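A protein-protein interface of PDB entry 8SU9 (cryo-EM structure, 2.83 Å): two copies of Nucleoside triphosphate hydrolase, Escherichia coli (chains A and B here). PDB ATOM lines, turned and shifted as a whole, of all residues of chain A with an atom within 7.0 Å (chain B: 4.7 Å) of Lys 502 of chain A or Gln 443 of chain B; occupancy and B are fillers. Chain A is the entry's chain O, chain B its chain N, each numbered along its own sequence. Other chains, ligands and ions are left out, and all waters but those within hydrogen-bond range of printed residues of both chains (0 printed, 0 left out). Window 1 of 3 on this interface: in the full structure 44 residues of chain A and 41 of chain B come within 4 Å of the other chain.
The side-chain carboxylate (OD2) of Asp 444 of chain B is in salt-bridge range of the guanidinium group (NE) of Arg 499 of chain A, at 2.8 Å. The side-chain amino group (NZ) of Lys 506 of chain A sits at hydrogen-bond distance from the backbone carbonyl oxygen (O) of Lys 439 of chain B, at 2.7 Å.
Glu 498 of chain A touches Gln 443 of chain B (OE2 to CB, 3.1 Å). Glu 498 of chain A touches Asp 444 of chain B (OE1 to OD1, 3.6 Å). His 445 of chain B touches Arg 499 of chain A. Lys 502 of chain A touches Lys 439 of chain B. CE of Lys 502 of chain A touches O of Leu 441 of chain B, 3.6 Å away. CD of Lys 502 of chain A touches CG of Gln 443 of chain B, 3.5 Å away.
Of the printed residues of chain B, Arg 499 of chain A touches Asp 444 and His 445. Of the printed residues of chain B, Lys 506 of chain A touches Lys 439 (2.7 Å). Printed residues of chain A within 4 Å of Leu 441 of chain B: Lys 502 (3.6 Å). Ala 442 of chain B touches none of the printed residues of chain A. Gln 443 of chain B touches just these residues of chain A: Glu 498 and Lys 502. Of the printed residues of chain A, Asp 444 of chain B touches Glu 498 (3.6 Å) and Arg 499 (2.8 Å). The nearest printed residue of chain A that does not touch Asp 444 of chain B is Lys 502 of chain A (6.9 Å).
Of the 13 printed residues of chain A, 4 touch a printed residue of chain B. Printed residues of chain A that touch a printed residue of chain B: Glu 498, Arg 499, Lys 502 and Lys 506. Hydrophobic or aromatic side chains of chain B that line the printed part of chain A: His 445. Among the printed residues, 8 pairs touch across the chains. Among the printed residues, Asp or Glu carboxylates within 4 Å of a Lys or Arg side-chain nitrogen of the other chain: Arg 499 of chain A with Asp 444 of chain B.
No position is printed for both chains.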
ATOM      1  N   HIS A 172       6.079 -22.820 -27.435  1.00  0.00           N
ATOM      2  CA  HIS A 172       5.848 -22.260 -28.756  1.00  0.00           C
ATOM      3  C   HIS A 172       6.060 -23.312 -29.842  1.00  0.00           C
ATOM      4  O   HIS A 172       6.794 -24.287 -29.667  1.00  0.00           O
ATOM      5  CB  HIS A 172       6.761 -21.060 -28.993  1.00  0.00           C
ATOM      6  CG  HIS A 172       6.642 -19.999 -27.945  1.00  0.00           C
ATOM      7  ND1 HIS A 172       5.490 -19.268 -27.755  1.00  0.00           N
ATOM      8  CD2 HIS A 172       7.531 -19.542 -27.034  1.00  0.00           C
ATOM      9  CE1 HIS A 172       5.672 -18.410 -26.769  1.00  0.00           C
ATOM     10  NE2 HIS A 172       6.903 -18.553 -26.315  1.00  0.00           N
ATOM     11  N   TYR A 497       8.532  -8.911 -30.224  1.00  0.00           N
ATOM     12  CA  TYR A 497       8.359 -10.355 -30.135  1.00  0.00           C
ATOM     13  C   TYR A 497       9.040 -10.946 -28.911  1.00  0.00           C
ATOM     14  O   TYR A 497       8.543 -11.926 -28.349  1.00  0.00           O
ATOM     15  CB  TYR A 497       8.888 -11.036 -31.397  1.00  0.00           C
ATOM     16  CG  TYR A 497       8.834 -12.546 -31.333  1.00  0.00           C
ATOM     17  CD1 TYR A 497       7.654 -13.229 -31.593  1.00  0.00           C
ATOM     18  CD2 TYR A 497       9.960 -13.287 -31.006  1.00  0.00           C
ATOM     19  CE1 TYR A 497       7.601 -14.608 -31.532  1.00  0.00           C
ATOM     20  CE2 TYR A 497       9.915 -14.664 -30.940  1.00  0.00           C
ATOM     21  CZ  TYR A 497       8.734 -15.319 -31.204  1.00  0.00           C
ATOM     22  OH  TYR A 497       8.686 -16.693 -31.142  1.00  0.00           O
ATOM     23  N   GLU A 498      10.169 -10.381 -28.487  1.00  0.00           N
ATOM     24  CA  GLU A 498      10.933 -10.985 -27.399  1.00  0.00           C
ATOM     25  C   GLU A 498      10.209 -10.828 -26.064  1.00  0.00           C
ATOM     26  O   GLU A 498      10.065 -11.797 -25.300  1.00  0.00           O
ATOM     27  CB  GLU A 498      12.328 -10.361 -27.358  1.00  0.00           C
ATOM     28  CG  GLU A 498      13.298 -11.003 -26.388  1.00  0.00           C
ATOM     29  CD  GLU A 498      14.691 -10.415 -26.508  1.00  0.00           C
ATOM     30  OE1 GLU A 498      14.879  -9.503 -27.340  1.00  0.00           O
ATOM     31  OE2 GLU A 498      15.601 -10.874 -25.788  1.00  0.00           O
ATOM     32  N   ARG A 499       9.733  -9.613 -25.773  1.00  0.00           N
ATOM     33  CA  ARG A 499       8.954  -9.391 -24.560  1.00  0.00           C
ATOM     34  C   ARG A 499       7.684 -10.228 -24.566  1.00  0.00           C
ATOM     35  O   ARG A 499       7.317 -10.820 -23.544  1.00  0.00           O
ATOM     36  CB  ARG A 499       8.608  -7.910 -24.416  1.00  0.00           C
ATOM     37  CG  ARG A 499       9.704  -7.050 -23.825  1.00  0.00           C
ATOM     38  CD  ARG A 499       9.144  -5.708 -23.386  1.00  0.00           C
ATOM     39  NE  ARG A 499      10.185  -4.706 -23.189  1.00  0.00           N
ATOM     40  CZ  ARG A 499       9.956  -3.452 -22.827  1.00  0.00           C
ATOM     41  NH1 ARG A 499       8.730  -3.010 -22.607  1.00  0.00           N
ATOM     42  NH2 ARG A 499      10.983  -2.620 -22.685  1.00  0.00           N
ATOM     43  N   LEU A 500       6.998 -10.283 -25.710  1.00  0.00           N
ATOM     44  CA  LEU A 500       5.773 -11.069 -25.801  1.00  0.00           C
ATOM     45  C   LEU A 500       6.050 -12.545 -25.564  1.00  0.00           C
ATOM     46  O   LEU A 500       5.283 -13.222 -24.874  1.00  0.00           O
ATOM     47  CB  LEU A 500       5.111 -10.854 -27.162  1.00  0.00           C
ATOM     48  CG  LEU A 500       3.783 -11.575 -27.399  1.00  0.00           C
ATOM     49  CD1 LEU A 500       2.753 -11.166 -26.365  1.00  0.00           C
ATOM     50  CD2 LEU A 500       3.273 -11.301 -28.801  1.00  0.00           C
ATOM     51  N   ALA A 501       7.152 -13.058 -26.114  1.00  0.00           N
ATOM     52  CA  ALA A 501       7.492 -14.464 -25.933  1.00  0.00           C
ATOM     53  C   ALA A 501       7.781 -14.779 -24.470  1.00  0.00           C
ATOM     54  O   ALA A 501       7.283 -15.773 -23.928  1.00  0.00           O
ATOM     55  CB  ALA A 501       8.689 -14.827 -26.810  1.00  0.00           C
ATOM     56  N   LYS A 502       8.582 -13.936 -23.810  1.00  0.00           N
ATOM     57  CA  LYS A 502       8.892 -14.190 -22.405  1.00  0.00           C
ATOM     58  C   LYS A 502       7.640 -14.101 -21.536  1.00  0.00           C
ATOM     59  O   LYS A 502       7.405 -14.958 -20.671  1.00  0.00           O
ATOM     60  CB  LYS A 502       9.957 -13.217 -21.908  1.00  0.00           C
ATOM     61  CG  LYS A 502      10.391 -13.480 -20.475  1.00  0.00           C
ATOM     62  CD  LYS A 502      11.494 -12.538 -20.037  1.00  0.00           C
ATOM     63  CE  LYS A 502      11.986 -12.868 -18.639  1.00  0.00           C
ATOM     64  NZ  LYS A 502      10.951 -12.592 -17.606  1.00  0.00           N
ATOM     65  N   GLU A 503       6.810 -13.079 -21.765  1.00  0.00           N
ATOM     66  CA  GLU A 503       5.596 -12.927 -20.971  1.00  0.00           C
ATOM     67  C   GLU A 503       4.614 -14.061 -21.222  1.00  0.00           C
ATOM     68  O   GLU A 503       3.903 -14.472 -20.302  1.00  0.00           O
ATOM     69  CB  GLU A 503       4.937 -11.581 -21.265  1.00  0.00           C
ATOM     70  CG  GLU A 503       5.732 -10.384 -20.778  1.00  0.00           C
ATOM     71  CD  GLU A 503       6.090 -10.485 -19.311  1.00  0.00           C
ATOM     72  OE1 GLU A 503       5.164 -10.519 -18.475  1.00  0.00           O
ATOM     73  OE2 GLU A 503       7.297 -10.532 -18.993  1.00  0.00           O
ATOM     74  N   GLY A 504       4.545 -14.567 -22.454  1.00  0.00           N
ATOM     75  CA  GLY A 504       3.689 -15.707 -22.722  1.00  0.00           C
ATOM     76  C   GLY A 504       4.186 -16.972 -22.056  1.00  0.00           C
ATOM     77  O   GLY A 504       3.395 -17.759 -21.529  1.00  0.00           O
ATOM     78  N   ARG A 505       5.502 -17.189 -22.070  1.00  0.00           N
ATOM     79  CA  ARG A 505       6.050 -18.355 -21.392  1.00  0.00           C
ATOM     80  C   ARG A 505       5.829 -18.276 -19.889  1.00  0.00           C
ATOM     81  O   ARG A 505       5.691 -19.309 -19.226  1.00  0.00           O
ATOM     82  CB  ARG A 505       7.537 -18.499 -21.710  1.00  0.00           C
ATOM     83  CG  ARG A 505       8.110 -19.867 -21.389  1.00  0.00           C
ATOM     84  CD  ARG A 505       9.603 -19.910 -21.659  1.00  0.00           C
ATOM     85  NE  ARG A 505       9.901 -19.930 -23.085  1.00  0.00           N
ATOM     86  CZ  ARG A 505       9.997 -21.032 -23.816  1.00  0.00           C
ATOM     87  NH1 ARG A 505       9.826 -22.231 -23.284  1.00  0.00           N
ATOM     88  NH2 ARG A 505      10.273 -20.929 -25.113  1.00  0.00           N
ATOM     89  N   LYS A 506       5.790 -17.065 -19.333  1.00  0.00           N
ATOM     90  CA  LYS A 506       5.553 -16.923 -17.901  1.00  0.00           C
ATOM     91  C   LYS A 506       4.076 -17.017 -17.523  1.00  0.00           C
ATOM     92  O   LYS A 506       3.732 -17.663 -16.529  1.00  0.00           O
ATOM     93  CB  LYS A 506       6.134 -15.597 -17.400  1.00  0.00           C
ATOM     94  CG  LYS A 506       7.607 -15.663 -17.057  1.00  0.00           C
ATOM     95  CD  LYS A 506       8.176 -14.280 -16.810  1.00  0.00           C
ATOM     96  CE  LYS A 506       7.494 -13.606 -15.637  1.00  0.00           C
ATOM     97  NZ  LYS A 506       8.188 -12.350 -15.248  1.00  0.00           N
ATOM     98  N   PHE A 507       3.190 -16.391 -18.298  1.00  0.00           N
ATOM     99  CA  PHE A 507       1.804 -16.169 -17.893  1.00  0.00           C
ATOM    100  C   PHE A 507       0.807 -16.784 -18.869  1.00  0.00           C
ATOM    101  O   PHE A 507      -0.194 -16.164 -19.229  1.00  0.00           O
ATOM    102  CB  PHE A 507       1.522 -14.678 -17.732  1.00  0.00           C
ATOM    103  CG  PHE A 507       2.385 -14.004 -16.706  1.00  0.00           C
ATOM    104  CD1 PHE A 507       2.470 -14.501 -15.418  1.00  0.00           C
ATOM    105  CD2 PHE A 507       3.103 -12.869 -17.028  1.00  0.00           C
ATOM    106  CE1 PHE A 507       3.263 -13.881 -14.475  1.00  0.00           C
ATOM    107  CE2 PHE A 507       3.895 -12.244 -16.090  1.00  0.00           C
ATOM    108  CZ  PHE A 507       3.974 -12.749 -14.812  1.00  0.00           C
ATOM    109  N   MET A 528      13.366 -19.781 -30.087  1.00  0.00           N
ATOM    110  CA  MET A 528      12.534 -19.764 -28.892  1.00  0.00           C
ATOM    111  C   MET A 528      11.485 -20.866 -28.887  1.00  0.00           C
ATOM    112  O   MET A 528      10.724 -20.973 -27.921  1.00  0.00           O
ATOM    113  CB  MET A 528      11.847 -18.403 -28.748  1.00  0.00           C
ATOM    114  CG  MET A 528      12.798 -17.234 -28.574  1.00  0.00           C
ATOM    115  SD  MET A 528      13.583 -17.186 -26.956  1.00  0.00           S
ATOM    116  CE  MET A 528      12.220 -16.628 -25.941  1.00  0.00           C
ATOM    117  N   LYS B 439      13.349 -12.671 -11.842  1.00  0.00           N
ATOM    118  CA  LYS B 439      12.205 -13.035 -12.666  1.00  0.00           C
ATOM    119  C   LYS B 439      11.406 -11.832 -13.154  1.00  0.00           C
ATOM    120  O   LYS B 439      10.529 -12.001 -14.007  1.00  0.00           O
ATOM    121  CB  LYS B 439      11.285 -13.978 -11.891  1.00  0.00           C
ATOM    122  CG  LYS B 439      10.306 -13.268 -10.979  1.00  0.00           C
ATOM    123  CD  LYS B 439       9.832 -14.179  -9.864  1.00  0.00           C
ATOM    124  CE  LYS B 439       9.025 -13.406  -8.836  1.00  0.00           C
ATOM    125  NZ  LYS B 439       8.920 -14.139  -7.545  1.00  0.00           N
ATOM    126  N   LEU B 441      12.746  -9.057 -14.612  1.00  0.00           N
ATOM    127  CA  LEU B 441      13.616  -8.256 -15.459  1.00  0.00           C
ATOM    128  C   LEU B 441      13.416  -8.637 -16.921  1.00  0.00           C
ATOM    129  O   LEU B 441      13.404  -9.821 -17.269  1.00  0.00           O
ATOM    130  CB  LEU B 441      15.073  -8.450 -15.030  1.00  0.00           C
ATOM    131  CG  LEU B 441      16.194  -7.582 -15.593  1.00  0.00           C
ATOM    132  CD1 LEU B 441      17.308  -7.458 -14.578  1.00  0.00           C
ATOM    133  CD2 LEU B 441      16.729  -8.194 -16.853  1.00  0.00           C
ATOM    134  N   ALA B 442      13.259  -7.627 -17.772  1.00  0.00           N
ATOM    135  CA  ALA B 442      12.923  -7.844 -19.172  1.00  0.00           C
ATOM    136  C   ALA B 442      14.127  -8.337 -19.966  1.00  0.00           C
ATOM    137  O   ALA B 442      15.280  -8.069 -19.621  1.00  0.00           O
ATOM    138  CB  ALA B 442      12.382  -6.560 -19.799  1.00  0.00           C
ATOM    139  N   GLN B 443      13.841  -9.058 -21.053  1.00  0.00           N
ATOM    140  CA  GLN B 443      14.897  -9.610 -21.897  1.00  0.00           C
ATOM    141  C   GLN B 443      15.723  -8.537 -22.589  1.00  0.00           C
ATOM    142  O   GLN B 443      16.829  -8.829 -23.055  1.00  0.00           O
ATOM    143  CB  GLN B 443      14.295 -10.538 -22.950  1.00  0.00           C
ATOM    144  CG  GLN B 443      13.922 -11.914 -22.448  1.00  0.00           C
ATOM    145  CD  GLN B 443      15.133 -12.739 -22.076  1.00  0.00           C
ATOM    146  OE1 GLN B 443      15.385 -13.001 -20.901  1.00  0.00           O
ATOM    147  NE2 GLN B 443      15.892 -13.156 -23.082  1.00  0.00           N
ATOM    148  N   ASP B 444      15.217  -7.309 -22.671  1.00  0.00           N
ATOM    149  CA  ASP B 444      15.921  -6.265 -23.404  1.00  0.00           C
ATOM    150  C   ASP B 444      17.006  -5.596 -22.570  1.00  0.00           C
ATOM    151  O   ASP B 444      17.941  -5.021 -23.135  1.00  0.00           O
ATOM    152  CB  ASP B 444      14.918  -5.221 -23.894  1.00  0.00           C
ATOM    153  CG  ASP B 444      13.691  -5.849 -24.516  1.00  0.00           C
ATOM    154  OD1 ASP B 444      13.812  -6.956 -25.076  1.00  0.00           O
ATOM    155  OD2 ASP B 444      12.603  -5.244 -24.427  1.00  0.00           O
ATOM    156  N   HIS B 445      16.911  -5.666 -21.244  1.00  0.00           N
ATOM    157  CA  HIS B 445      17.836  -4.967 -20.362  1.00  0.00           C
ATOM    158  C   HIS B 445      18.757  -5.894 -19.582  1.00  0.00           C
ATOM    159  O   HIS B 445      19.584  -5.405 -18.805  1.00  0.00           O
ATOM    160  CB  HIS B 445      17.061  -4.081 -19.379  1.00  0.00           C
ATOM    161  CG  HIS B 445      15.943  -3.309 -20.006  1.00  0.00           C
ATOM    162  ND1 HIS B 445      16.124  -2.493 -21.101  1.00  0.00           N
ATOM    163  CD2 HIS B 445      14.631  -3.221 -19.684  1.00  0.00           C
ATOM    164  CE1 HIS B 445      14.970  -1.940 -21.430  1.00  0.00           C
ATOM    165  NE2 HIS B 445      14.048  -2.365 -20.585  1.00  0.00           N
ATOM    166  N   ALA B 446      18.637  -7.209 -19.755  1.00  0.00           N
ATOM    167  CA  ALA B 446      19.503  -8.132 -19.022  1.00  0.00           C
ATOM    168  C   ALA B 446      20.982  -7.970 -19.353  1.00  0.00           C
ATOM    169  O   ALA B 446      21.792  -7.850 -18.413  1.00  0.00           O
ATOM    170  CB  ALA B 446      19.032  -9.572 -19.258  1.00  0.00           C
ATOM    171  N   PRO B 447      21.412  -7.959 -20.625  1.00  0.00           N
ATOM    172  CA  PRO B 447      22.861  -7.892 -20.886  1.00  0.00           C
ATOM    173  C   PRO B 447      23.523  -6.657 -20.306  1.00  0.00           C
ATOM    174  O   PRO B 447      24.560  -6.772 -19.640  1.00  0.00           O
ATOM    175  CB  PRO B 447      22.938  -7.918 -22.418  1.00  0.00           C
ATOM    176  CG  PRO B 447      21.672  -8.536 -22.858  1.00  0.00           C
ATOM    177  CD  PRO B 447      20.645  -8.098 -21.877  1.00  0.00           C
